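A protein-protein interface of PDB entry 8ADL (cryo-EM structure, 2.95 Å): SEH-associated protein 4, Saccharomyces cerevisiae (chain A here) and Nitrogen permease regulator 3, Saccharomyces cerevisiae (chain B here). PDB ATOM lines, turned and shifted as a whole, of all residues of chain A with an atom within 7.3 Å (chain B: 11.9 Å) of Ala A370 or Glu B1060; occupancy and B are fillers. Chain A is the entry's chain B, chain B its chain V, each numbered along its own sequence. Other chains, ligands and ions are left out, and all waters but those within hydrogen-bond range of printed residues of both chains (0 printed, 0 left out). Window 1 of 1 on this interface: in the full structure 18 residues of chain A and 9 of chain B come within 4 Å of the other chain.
CB of Asp B1063 touches O of Pro A23, 3.4 Å away.
Gly A294 touches Tyr B1061.
Glu B1060 touches Asn A304.
Asp B1062 touches Asn A304.
Glu B1060 touches Arg A368 (OE2 to CA, 3.7 Å).
Glu B1060 touches Ala A370 (O to CB, 3.8 Å).
O of Gln A389 touches SD of Met B966 (3.9 Å).
Gln A389 touches Phe B1059 (NE2 to O, 3.6 Å).
Gln A389 touches Glu B1060.
Ser A390 touches Met B966 (CB to CB, 3.4 Å).
No residue of chain B comes within 4 Å of Ser A305.
No residue of chain B comes within 4 Å of Leu A320.
Asp A367 touches none of the printed residues of chain B.
Arg A368 touches one residue of chain B.
No residue of chain B comes within 4 Å of Val A369.
Of chain B, only Glu B1060 comes within 4 Å of Ala A370.
Gln A389 touches just these residues of chain B: Met B966 (3.9 Å), Phe B1059 (3.6 Å) and Glu B1060 (3.95 Å).
Of the printed residues of chain B, Ser A390 touches Met B966 (3.4 Å).
Of the printed residues of chain A, Glu B1060 touches Asn A304 (3.6 Å), Arg A322 (3.2 Å), Gly A323 (3.5 Å), Arg A368 (3.7 Å), Ala A370 (3.8 Å) and Gln A389 (3.95 Å).
Printed residues of chain A within 4 Å of Asp B1062: Asn A304 (3.5 Å).
The nearest residue of chain B that does not touch Ala A370 is Asp B1063 (4.5 Å).
The backbone NH (N) of Gln A389 lies within hydrogen-bond range of the backbone carbonyl oxygen (O) of Arg A368 (2.7 Å).
The backbone NH (N) of Arg A368 is in hydrogen-bond range of the backbone carbonyl oxygen (O) of Gly A323, at 3.4 Å.
The side-chain sulfur (SG) of Cys A306 lies within hydrogen-bond range of the backbone NH (N) of Gly A294, 3.8 Å away.
The side-chain amide nitrogen of Asn A304 sits at hydrogen-bond distance from the backbone carbonyl oxygen of Gly A2 (2.8 Å).
O of Met A387 sits at hydrogen-bond distance from N of Ala A370, 3.1 Å away.
N of Phe B1059 sits at hydrogen-bond distance from OD1 of Asp B1062 (2.9 Å).
Among the printed residues, 16 pairs touch across the chains.
The backbone NH (N) of Gly A323 is in hydrogen-bond range of the side-chain carboxylate (OE1) of Glu B1060 (3.5 Å).
The side-chain carboxylate of Asp B1063 lies within hydrogen-bond range of the side-chain amide nitrogen of Asn A304 (2.8 Å).
The backbone NH of Gly A2 sits close to the side-chain carboxylate of Asp B1063 (2.3 Å).
The backbone carbonyl oxygen of Tyr B1061 sits at hydrogen-bond distance from the backbone NH of Asn A304.
The backbone carbonyl oxygen (O) of Arg A322 sits close to the side-chain carboxylate (OE1) of Glu B1060, 3.2 Å away.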
ATOM      1  N   GLY A   2      34.864 -26.316  -5.846  1.00  0.00           N
ATOM      2  CA  GLY A   2      34.842 -24.890  -6.115  1.00  0.00           C
ATOM      3  C   GLY A   2      35.260 -24.052  -4.924  1.00  0.00           C
ATOM      4  O   GLY A   2      34.715 -24.194  -3.831  1.00  0.00           O
ATOM      5  N   PRO A  23      35.114 -26.355 -10.310  1.00  0.00           N
ATOM      6  CA  PRO A  23      34.710 -27.535  -9.522  1.00  0.00           C
ATOM      7  C   PRO A  23      35.472 -28.807  -9.857  1.00  0.00           C
ATOM      8  O   PRO A  23      35.514 -29.721  -9.024  1.00  0.00           O
ATOM      9  CB  PRO A  23      33.219 -27.680  -9.851  1.00  0.00           C
ATOM     10  CG  PRO A  23      32.785 -26.305 -10.199  1.00  0.00           C
ATOM     11  CD  PRO A  23      33.948 -25.682 -10.913  1.00  0.00           C
ATOM     12  N   GLY A 294      28.124 -28.861   5.532  1.00  0.00           N
ATOM     13  CA  GLY A 294      28.149 -30.155   4.885  1.00  0.00           C
ATOM     14  C   GLY A 294      29.014 -31.153   5.630  1.00  0.00           C
ATOM     15  O   GLY A 294      29.930 -30.803   6.374  1.00  0.00           O
ATOM     16  N   MET A 303      36.096 -29.998  -0.624  1.00  0.00           N
ATOM     17  CA  MET A 303      34.873 -29.511  -0.003  1.00  0.00           C
ATOM     18  C   MET A 303      34.674 -28.025  -0.247  1.00  0.00           C
ATOM     19  O   MET A 303      35.616 -27.233  -0.157  1.00  0.00           O
ATOM     20  CB  MET A 303      34.861 -29.777   1.502  1.00  0.00           C
ATOM     21  CG  MET A 303      34.515 -31.202   1.867  1.00  0.00           C
ATOM     22  SD  MET A 303      33.919 -31.316   3.558  1.00  0.00           S
ATOM     23  CE  MET A 303      32.335 -30.498   3.409  1.00  0.00           C
ATOM     24  N   ASN A 304      33.434 -27.664  -0.555  1.00  0.00           N
ATOM     25  CA  ASN A 304      33.066 -26.279  -0.788  1.00  0.00           C
ATOM     26  C   ASN A 304      32.830 -25.592   0.549  1.00  0.00           C
ATOM     27  O   ASN A 304      32.100 -26.110   1.401  1.00  0.00           O
ATOM     28  CB  ASN A 304      31.810 -26.201  -1.652  1.00  0.00           C
ATOM     29  CG  ASN A 304      32.026 -26.753  -3.042  1.00  0.00           C
ATOM     30  OD1 ASN A 304      31.785 -27.931  -3.300  1.00  0.00           O
ATOM     31  ND2 ASN A 304      32.472 -25.898  -3.951  1.00  0.00           N
ATOM     32  N   SER A 305      33.450 -24.433   0.740  1.00  0.00           N
ATOM     33  CA  SER A 305      33.294 -23.686   1.987  1.00  0.00           C
ATOM     34  C   SER A 305      31.928 -23.017   1.965  1.00  0.00           C
ATOM     35  O   SER A 305      31.726 -22.005   1.290  1.00  0.00           O
ATOM     36  CB  SER A 305      34.416 -22.668   2.148  1.00  0.00           C
ATOM     37  OG  SER A 305      34.576 -21.903   0.968  1.00  0.00           O
ATOM     38  N   CYS A 306      30.980 -23.586   2.711  1.00  0.00           N
ATOM     39  CA  CYS A 306      29.623 -23.064   2.801  1.00  0.00           C
ATOM     40  C   CYS A 306      29.409 -22.229   4.057  1.00  0.00           C
ATOM     41  O   CYS A 306      28.314 -22.233   4.629  1.00  0.00           O
ATOM     42  CB  CYS A 306      28.614 -24.211   2.746  1.00  0.00           C
ATOM     43  SG  CYS A 306      28.935 -25.547   3.915  1.00  0.00           S
ATOM     44  N   PHE A 307      30.441 -21.508   4.493  1.00  0.00           N
ATOM     45  CA  PHE A 307      30.358 -20.670   5.681  1.00  0.00           C
ATOM     46  C   PHE A 307      31.438 -19.603   5.595  1.00  0.00           C
ATOM     47  O   PHE A 307      32.616 -19.927   5.427  1.00  0.00           O
ATOM     48  CB  PHE A 307      30.508 -21.507   6.954  1.00  0.00           C
ATOM     49  CG  PHE A 307      31.099 -20.760   8.107  1.00  0.00           C
ATOM     50  CD1 PHE A 307      30.355 -19.825   8.806  1.00  0.00           C
ATOM     51  CD2 PHE A 307      32.398 -21.011   8.507  1.00  0.00           C
ATOM     52  CE1 PHE A 307      30.905 -19.142   9.871  1.00  0.00           C
ATOM     53  CE2 PHE A 307      32.947 -20.334   9.563  1.00  0.00           C
ATOM     54  CZ  PHE A 307      32.201 -19.397  10.249  1.00  0.00           C
ATOM     55  N   LEU A 320      25.589 -21.392   3.949  1.00  0.00           N
ATOM     56  CA  LEU A 320      24.910 -21.832   2.738  1.00  0.00           C
ATOM     57  C   LEU A 320      24.205 -23.152   3.013  1.00  0.00           C
ATOM     58  O   LEU A 320      24.835 -24.114   3.463  1.00  0.00           O
ATOM     59  CB  LEU A 320      25.901 -21.990   1.583  1.00  0.00           C
ATOM     60  CG  LEU A 320      25.335 -22.298   0.198  1.00  0.00           C
ATOM     61  CD1 LEU A 320      24.600 -21.099  -0.364  1.00  0.00           C
ATOM     62  CD2 LEU A 320      26.448 -22.728  -0.737  1.00  0.00           C
ATOM     63  N   HIS A 321      22.902 -23.196   2.742  1.00  0.00           N
ATOM     64  CA  HIS A 321      22.077 -24.355   3.059  1.00  0.00           C
ATOM     65  C   HIS A 321      21.358 -24.821   1.803  1.00  0.00           C
ATOM     66  O   HIS A 321      20.564 -24.068   1.230  1.00  0.00           O
ATOM     67  CB  HIS A 321      21.067 -24.028   4.160  1.00  0.00           C
ATOM     68  CG  HIS A 321      21.696 -23.610   5.450  1.00  0.00           C
ATOM     69  ND1 HIS A 321      22.279 -24.507   6.318  1.00  0.00           N
ATOM     70  CD2 HIS A 321      21.836 -22.390   6.020  1.00  0.00           C
ATOM     71  CE1 HIS A 321      22.749 -23.859   7.367  1.00  0.00           C
ATOM     72  NE2 HIS A 321      22.494 -22.573   7.212  1.00  0.00           N
ATOM     73  N   ARG A 322      21.660 -26.049   1.374  1.00  0.00           N
ATOM     74  CA  ARG A 322      20.993 -26.752   0.275  1.00  0.00           C
ATOM     75  C   ARG A 322      21.108 -26.030  -1.067  1.00  0.00           C
ATOM     76  O   ARG A 322      20.339 -26.312  -1.990  1.00  0.00           O
ATOM     77  CB  ARG A 322      19.519 -27.022   0.605  1.00  0.00           C
ATOM     78  CG  ARG A 322      19.310 -28.129   1.624  1.00  0.00           C
ATOM     79  CD  ARG A 322      17.950 -28.015   2.290  1.00  0.00           C
ATOM     80  NE  ARG A 322      17.771 -26.717   2.928  1.00  0.00           N
ATOM     81  CZ  ARG A 322      16.658 -26.325   3.532  1.00  0.00           C
ATOM     82  NH1 ARG A 322      15.595 -27.109   3.600  1.00  0.00           N
ATOM     83  NH2 ARG A 322      16.611 -25.115   4.083  1.00  0.00           N
ATOM     84  N   GLY A 323      22.054 -25.102  -1.202  1.00  0.00           N
ATOM     85  CA  GLY A 323      22.235 -24.380  -2.445  1.00  0.00           C
ATOM     86  C   GLY A 323      21.128 -23.421  -2.815  1.00  0.00           C
ATOM     87  O   GLY A 323      21.091 -22.958  -3.958  1.00  0.00           O
ATOM     88  N   ASP A 324      20.229 -23.101  -1.892  1.00  0.00           N
ATOM     89  CA  ASP A 324      19.081 -22.258  -2.198  1.00  0.00           C
ATOM     90  C   ASP A 324      18.980 -21.023  -1.320  1.00  0.00           C
ATOM     91  O   ASP A 324      18.594 -19.958  -1.809  1.00  0.00           O
ATOM     92  CB  ASP A 324      17.783 -23.070  -2.075  1.00  0.00           C
ATOM     93  CG  ASP A 324      17.608 -24.065  -3.205  1.00  0.00           C
ATOM     94  OD1 ASP A 324      18.298 -23.922  -4.237  1.00  0.00           O
ATOM     95  OD2 ASP A 324      16.779 -24.988  -3.063  1.00  0.00           O
ATOM     96  N   ASP A 367      19.701 -21.656  -8.285  1.00  0.00           N
ATOM     97  CA  ASP A 367      19.894 -22.789  -7.396  1.00  0.00           C
ATOM     98  C   ASP A 367      21.245 -23.453  -7.662  1.00  0.00           C
ATOM     99  O   ASP A 367      22.035 -23.006  -8.501  1.00  0.00           O
ATOM    100  CB  ASP A 367      18.752 -23.788  -7.556  1.00  0.00           C
ATOM    101  CG  ASP A 367      17.390 -23.152  -7.361  1.00  0.00           C
ATOM    102  OD1 ASP A 367      17.333 -21.930  -7.112  1.00  0.00           O
ATOM    103  OD2 ASP A 367      16.376 -23.876  -7.455  1.00  0.00           O
ATOM    104  N   ARG A 368      21.495 -24.544  -6.927  1.00  0.00           N
ATOM    105  CA  ARG A 368      22.686 -25.392  -7.063  1.00  0.00           C
ATOM    106  C   ARG A 368      23.975 -24.595  -6.853  1.00  0.00           C
ATOM    107  O   ARG A 368      24.932 -24.697  -7.623  1.00  0.00           O
ATOM    108  CB  ARG A 368      22.700 -26.128  -8.407  1.00  0.00           C
ATOM    109  CG  ARG A 368      21.694 -27.265  -8.494  1.00  0.00           C
ATOM    110  CD  ARG A 368      21.623 -27.853  -9.892  1.00  0.00           C
ATOM    111  NE  ARG A 368      20.582 -28.868  -9.999  1.00  0.00           N
ATOM    112  CZ  ARG A 368      20.155 -29.390 -11.141  1.00  0.00           C
ATOM    113  NH1 ARG A 368      20.661 -29.013 -12.305  1.00  0.00           N
ATOM    114  NH2 ARG A 368      19.198 -30.312 -11.116  1.00  0.00           N
ATOM    115  N   VAL A 369      23.990 -23.793  -5.793  1.00  0.00           N
ATOM    116  CA  VAL A 369      25.163 -23.012  -5.421  1.00  0.00           C
ATOM    117  C   VAL A 369      26.022 -23.852  -4.488  1.00  0.00           C
ATOM    118  O   VAL A 369      25.530 -24.383  -3.486  1.00  0.00           O
ATOM    119  CB  VAL A 369      24.754 -21.685  -4.759  1.00  0.00           C
ATOM    120  CG1 VAL A 369      25.974 -20.951  -4.229  1.00  0.00           C
ATOM    121  CG2 VAL A 369      24.009 -20.816  -5.748  1.00  0.00           C
ATOM    122  N   ALA A 370      27.304 -23.984  -4.820  1.00  0.00           N
ATOM    123  CA  ALA A 370      28.231 -24.751  -3.999  1.00  0.00           C
ATOM    124  C   ALA A 370      29.022 -23.894  -3.022  1.00  0.00           C
ATOM    125  O   ALA A 370      29.196 -24.289  -1.866  1.00  0.00           O
ATOM    126  CB  ALA A 370      29.201 -25.532  -4.892  1.00  0.00           C
ATOM    127  N   THR A 371      29.484 -22.719  -3.444  1.00  0.00           N
ATOM    128  CA  THR A 371      30.274 -21.860  -2.576  1.00  0.00           C
ATOM    129  C   THR A 371      29.977 -20.405  -2.905  1.00  0.00           C
ATOM    130  O   THR A 371      29.412 -20.087  -3.954  1.00  0.00           O
ATOM    131  CB  THR A 371      31.775 -22.149  -2.709  1.00  0.00           C
ATOM    132  OG1 THR A 371      32.505 -21.335  -1.784  1.00  0.00           O
ATOM    133  CG2 THR A 371      32.252 -21.860  -4.121  1.00  0.00           C
ATOM    134  N   PHE A 372      30.366 -19.522  -1.989  1.00  0.00           N
ATOM    135  CA  PHE A 372      30.045 -18.105  -2.105  1.00  0.00           C
ATOM    136  C   PHE A 372      31.051 -17.301  -1.295  1.00  0.00           C
ATOM    137  O   PHE A 372      31.808 -17.846  -0.488  1.00  0.00           O
ATOM    138  CB  PHE A 372      28.616 -17.812  -1.634  1.00  0.00           C
ATOM    139  CG  PHE A 372      28.469 -17.751  -0.139  1.00  0.00           C
ATOM    140  CD1 PHE A 372      28.576 -18.897   0.634  1.00  0.00           C
ATOM    141  CD2 PHE A 372      28.224 -16.544   0.494  1.00  0.00           C
ATOM    142  CE1 PHE A 372      28.442 -18.838   2.006  1.00  0.00           C
ATOM    143  CE2 PHE A 372      28.090 -16.479   1.865  1.00  0.00           C
ATOM    144  CZ  PHE A 372      28.200 -17.628   2.621  1.00  0.00           C
ATOM    145  N   CYS A 386      28.721 -15.680  -5.996  1.00  0.00           N
ATOM    146  CA  CYS A 386      28.391 -17.080  -5.794  1.00  0.00           C
ATOM    147  C   CYS A 386      28.859 -17.897  -6.986  1.00  0.00           C
ATOM    148  O   CYS A 386      28.740 -17.463  -8.136  1.00  0.00           O
ATOM    149  CB  CYS A 386      26.885 -17.268  -5.590  1.00  0.00           C
ATOM    150  SG  CYS A 386      26.201 -16.354  -4.189  1.00  0.00           S
ATOM    151  N   MET A 387      29.390 -19.081  -6.704  1.00  0.00           N
ATOM    152  CA  MET A 387      29.832 -20.019  -7.725  1.00  0.00           C
ATOM    153  C   MET A 387      28.899 -21.219  -7.690  1.00  0.00           C
ATOM    154  O   MET A 387      28.725 -21.843  -6.637  1.00  0.00           O
ATOM    155  CB  MET A 387      31.281 -20.446  -7.489  1.00  0.00           C
ATOM    156  CG  MET A 387      31.669 -21.745  -8.172  1.00  0.00           C
ATOM    157  SD  MET A 387      33.429 -22.097  -8.024  1.00  0.00           S
ATOM    158  CE  MET A 387      34.041 -21.398  -9.554  1.00  0.00           C
ATOM    159  N   ARG A 388      28.300 -21.537  -8.832  1.00  0.00           N
ATOM    160  CA  ARG A 388      27.334 -22.618  -8.883  1.00  0.00           C
ATOM    161  C   ARG A 388      28.052 -23.962  -8.973  1.00  0.00           C
ATOM    162  O   ARG A 388      29.284 -24.040  -9.015  1.00  0.00           O
ATOM    163  CB  ARG A 388      26.383 -22.414 -10.059  1.00  0.00           C
ATOM    164  CG  ARG A 388      25.759 -21.028 -10.103  1.00  0.00           C
ATOM    165  CD  ARG A 388      24.769 -20.895 -11.244  1.00  0.00           C
ATOM    166  NE  ARG A 388      23.653 -21.823 -11.116  1.00  0.00           N
ATOM    167  CZ  ARG A 388      22.627 -21.879 -11.954  1.00  0.00           C
ATOM    168  NH1 ARG A 388      22.539 -21.065 -12.993  1.00  0.00           N
ATOM    169  NH2 ARG A 388      21.663 -22.770 -11.742  1.00  0.00           N
ATOM    170  N   GLN A 389      27.266 -25.040  -8.993  1.00  0.00           N
ATOM    171  CA  GLN A 389      27.839 -26.380  -9.066  1.00  0.00           C
ATOM    172  C   GLN A 389      28.474 -26.639 -10.428  1.00  0.00           C
ATOM    173  O   GLN A 389      29.425 -27.423 -10.533  1.00  0.00           O
ATOM    174  CB  GLN A 389      26.761 -27.416  -8.737  1.00  0.00           C
ATOM    175  CG  GLN A 389      27.247 -28.854  -8.651  1.00  0.00           C
ATOM    176  CD  GLN A 389      26.144 -29.816  -8.260  1.00  0.00           C
ATOM    177  OE1 GLN A 389      24.994 -29.418  -8.076  1.00  0.00           O
ATOM    178  NE2 GLN A 389      26.491 -31.091  -8.125  1.00  0.00           N
ATOM    179  N   SER A 390      27.991 -25.966 -11.469  1.00  0.00           N
ATOM    180  CA  SER A 390      28.533 -26.096 -12.815  1.00  0.00           C
ATOM    181  C   SER A 390      29.717 -25.173 -13.071  1.00  0.00           C
ATOM    182  O   SER A 390      30.257 -25.177 -14.182  1.00  0.00           O
ATOM    183  CB  SER A 390      27.438 -25.823 -13.851  1.00  0.00           C
ATOM    184  OG  SER A 390      26.985 -24.484 -13.770  1.00  0.00           O
ATOM    185  N   LYS B 962      29.604 -34.323 -17.683  1.00  0.00           N
ATOM    186  CA  LYS B 962      28.633 -33.633 -16.838  1.00  0.00           C
ATOM    187  C   LYS B 962      28.688 -32.117 -16.990  1.00  0.00           C
ATOM    188  O   LYS B 962      27.680 -31.445 -16.747  1.00  0.00           O
ATOM    189  CB  LYS B 962      28.836 -34.015 -15.369  1.00  0.00           C
ATOM    190  CG  LYS B 962      30.199 -33.655 -14.801  1.00  0.00           C
ATOM    191  CD  LYS B 962      30.168 -33.594 -13.282  1.00  0.00           C
ATOM    192  CE  LYS B 962      30.035 -34.977 -12.671  1.00  0.00           C
ATOM    193  NZ  LYS B 962      30.227 -34.955 -11.194  1.00  0.00           N
ATOM    194  N   MET B 966      25.507 -29.683 -17.520  1.00  0.00           N
ATOM    195  CA  MET B 966      25.174 -28.591 -16.610  1.00  0.00           C
ATOM    196  C   MET B 966      25.103 -27.254 -17.337  1.00  0.00           C
ATOM    197  O   MET B 966      24.253 -26.415 -17.015  1.00  0.00           O
ATOM    198  CB  MET B 966      26.190 -28.537 -15.472  1.00  0.00           C
ATOM    199  CG  MET B 966      26.045 -29.655 -14.457  1.00  0.00           C
ATOM    200  SD  MET B 966      27.060 -29.395 -12.992  1.00  0.00           S
ATOM    201  CE  MET B 966      26.810 -30.944 -12.128  1.00  0.00           C
ATOM    202  N   ASP B 969      21.810 -27.300 -19.113  1.00  0.00           N
ATOM    203  CA  ASP B 969      20.749 -27.049 -18.140  1.00  0.00           C
ATOM    204  C   ASP B 969      20.677 -25.574 -17.765  1.00  0.00           C
ATOM    205  O   ASP B 969      19.584 -25.024 -17.591  1.00  0.00           O
ATOM    206  CB  ASP B 969      20.960 -27.907 -16.893  1.00  0.00           C
ATOM    207  CG  ASP B 969      20.733 -29.382 -17.154  1.00  0.00           C
ATOM    208  OD1 ASP B 969      20.198 -29.722 -18.230  1.00  0.00           O
ATOM    209  OD2 ASP B 969      21.091 -30.202 -16.283  1.00  0.00           O
ATOM    210  N   PHE B1059      27.719 -34.444  -3.799  1.00  0.00           N
ATOM    211  CA  PHE B1059      26.550 -33.576  -3.739  1.00  0.00           C
ATOM    212  C   PHE B1059      26.938 -32.118  -3.958  1.00  0.00           C
ATOM    213  O   PHE B1059      27.709 -31.801  -4.863  1.00  0.00           O
ATOM    214  CB  PHE B1059      25.833 -33.735  -2.398  1.00  0.00           C
ATOM    215  CG  PHE B1059      24.948 -34.942  -2.323  1.00  0.00           C
ATOM    216  CD1 PHE B1059      25.457 -36.168  -1.927  1.00  0.00           C
ATOM    217  CD2 PHE B1059      23.606 -34.853  -2.654  1.00  0.00           C
ATOM    218  CE1 PHE B1059      24.643 -37.285  -1.859  1.00  0.00           C
ATOM    219  CE2 PHE B1059      22.784 -35.966  -2.589  1.00  0.00           C
ATOM    220  CZ  PHE B1059      23.305 -37.182  -2.191  1.00  0.00           C
ATOM    221  N   GLU B1060      26.395 -31.233  -3.122  1.00  0.00           N
ATOM    222  CA  GLU B1060      26.674 -29.808  -3.220  1.00  0.00           C
ATOM    223  C   GLU B1060      27.727 -29.329  -2.233  1.00  0.00           C
ATOM    224  O   GLU B1060      28.313 -28.262  -2.449  1.00  0.00           O
ATOM    225  CB  GLU B1060      25.386 -29.005  -3.009  1.00  0.00           C
ATOM    226  CG  GLU B1060      24.431 -29.070  -4.180  1.00  0.00           C
ATOM    227  CD  GLU B1060      23.088 -28.460  -3.863  1.00  0.00           C
ATOM    228  OE1 GLU B1060      22.833 -28.171  -2.675  1.00  0.00           O
ATOM    229  OE2 GLU B1060      22.284 -28.269  -4.799  1.00  0.00           O
ATOM    230  N   TYR B1061      27.983 -30.080  -1.163  1.00  0.00           N
ATOM    231  CA  TYR B1061      29.000 -29.691  -0.198  1.00  0.00           C
ATOM    232  C   TYR B1061      30.404 -30.121  -0.599  1.00  0.00           C
ATOM    233  O   TYR B1061      31.371 -29.675   0.028  1.00  0.00           O
ATOM    234  CB  TYR B1061      28.662 -30.266   1.180  1.00  0.00           C
ATOM    235  CG  TYR B1061      28.134 -31.684   1.157  1.00  0.00           C
ATOM    236  CD1 TYR B1061      28.998 -32.767   1.062  1.00  0.00           C
ATOM    237  CD2 TYR B1061      26.770 -31.938   1.245  1.00  0.00           C
ATOM    238  CE1 TYR B1061      28.519 -34.065   1.044  1.00  0.00           C
ATOM    239  CE2 TYR B1061      26.281 -33.232   1.228  1.00  0.00           C
ATOM    240  CZ  TYR B1061      27.160 -34.290   1.128  1.00  0.00           C
ATOM    241  OH  TYR B1061      26.677 -35.579   1.112  1.00  0.00           O
ATOM    242  N   ASP B1062      30.543 -30.965  -1.618  1.00  0.00           N
ATOM    243  CA  ASP B1062      31.849 -31.413  -2.079  1.00  0.00           C
ATOM    244  C   ASP B1062      31.892 -31.410  -3.603  1.00  0.00           C
ATOM    245  O   ASP B1062      30.858 -31.453  -4.273  1.00  0.00           O
ATOM    246  CB  ASP B1062      32.207 -32.790  -1.480  1.00  0.00           C
ATOM    247  CG  ASP B1062      31.225 -33.898  -1.858  1.00  0.00           C
ATOM    248  OD1 ASP B1062      30.214 -33.646  -2.544  1.00  0.00           O
ATOM    249  OD2 ASP B1062      31.467 -35.049  -1.445  1.00  0.00           O
ATOM    250  N   ASP B1063      33.107 -31.340  -4.146  1.00  0.00           N
ATOM    251  CA  ASP B1063      33.332 -31.329  -5.592  1.00  0.00           C
ATOM    252  C   ASP B1063      34.343 -32.403  -5.970  1.00  0.00           C
ATOM    253  O   ASP B1063      35.526 -32.107  -6.181  1.00  0.00           O
ATOM    254  CB  ASP B1063      33.815 -29.961  -6.075  1.00  0.00           C
ATOM    255  CG  ASP B1063      32.708 -28.931  -6.107  1.00  0.00           C
ATOM    256  OD1 ASP B1063      31.536 -29.318  -6.298  1.00  0.00           O
ATOM    257  OD2 ASP B1063      33.013 -27.729  -5.956  1.00  0.00           O
ATOM    258  N   PRO B1064      33.913 -33.661  -6.081  1.00  0.00           N
ATOM    259  CA  PRO B1064      34.844 -34.713  -6.512  1.00  0.00           C
ATOM    260  C   PRO B1064      35.063 -34.640  -8.017  1.00  0.00           C
ATOM    261  O   PRO B1064      34.110 -34.536  -8.793  1.00  0.00           O
ATOM    262  CB  PRO B1064      34.137 -36.010  -6.105  1.00  0.00           C
ATOM    263  CG  PRO B1064      32.685 -35.664  -6.069  1.00  0.00           C
ATOM    264  CD  PRO B1064      32.553 -34.178  -5.840  1.00  0.00           C
ATOM    265  N   GLU B1065      36.326 -34.686  -8.425  1.00  0.00           N
ATOM    266  CA  GLU B1065      36.692 -34.588  -9.831  1.00  0.00           C
ATOM    267  C   GLU B1065      36.918 -35.944 -10.488  1.00  0.00           C
ATOM    268  O   GLU B1065      37.265 -35.993 -11.671  1.00  0.00           O
ATOM    269  CB  GLU B1065      37.928 -33.686  -9.982  1.00  0.00           C
ATOM    270  CG  GLU B1065      39.187 -34.143  -9.240  1.00  0.00           C
ATOM    271  CD  GLU B1065      40.073 -35.072 -10.052  1.00  0.00           C
ATOM    272  OE1 GLU B1065      39.953 -35.082 -11.294  1.00  0.00           O
ATOM    273  OE2 GLU B1065      40.900 -35.783  -9.443  1.00  0.00           O
ATOM    274  N   GLN B1067      34.415 -38.421 -10.421  1.00  0.00           N
ATOM    275  CA  GLN B1067      33.075 -38.998 -10.409  1.00  0.00           C
ATOM    276  C   GLN B1067      32.236 -38.413 -11.536  1.00  0.00           C
ATOM    277  O   GLN B1067      31.111 -37.951 -11.331  1.00  0.00           O
ATOM    278  CB  GLN B1067      32.396 -38.774  -9.061  1.00  0.00           C
ATOM    279  CG  GLN B1067      31.518 -39.929  -8.610  1.00  0.00           C
ATOM    280  CD  GLN B1067      30.884 -39.681  -7.255  1.00  0.00           C
ATOM    281  OE1 GLN B1067      30.858 -38.551  -6.766  1.00  0.00           O
ATOM    282  NE2 GLN B1067      30.369 -40.739  -6.641  1.00  0.00           N
ATOM    283  N   ASP B1069      29.853 -37.932 -14.755  1.00  0.00           N
ATOM    284  CA  ASP B1069      28.612 -38.505 -15.271  1.00  0.00           C
ATOM    285  C   ASP B1069      28.680 -38.376 -16.790  1.00  0.00           C
ATOM    286  O   ASP B1069      28.188 -37.403 -17.364  1.00  0.00           O
ATOM    287  CB  ASP B1069      27.379 -37.803 -14.698  1.00  0.00           C
ATOM    288  CG  ASP B1069      27.388 -37.741 -13.182  1.00  0.00           C
ATOM    289  OD1 ASP B1069      28.305 -38.315 -12.559  1.00  0.00           O
ATOM    290  OD2 ASP B1069      26.472 -37.115 -12.610  1.00  0.00           O
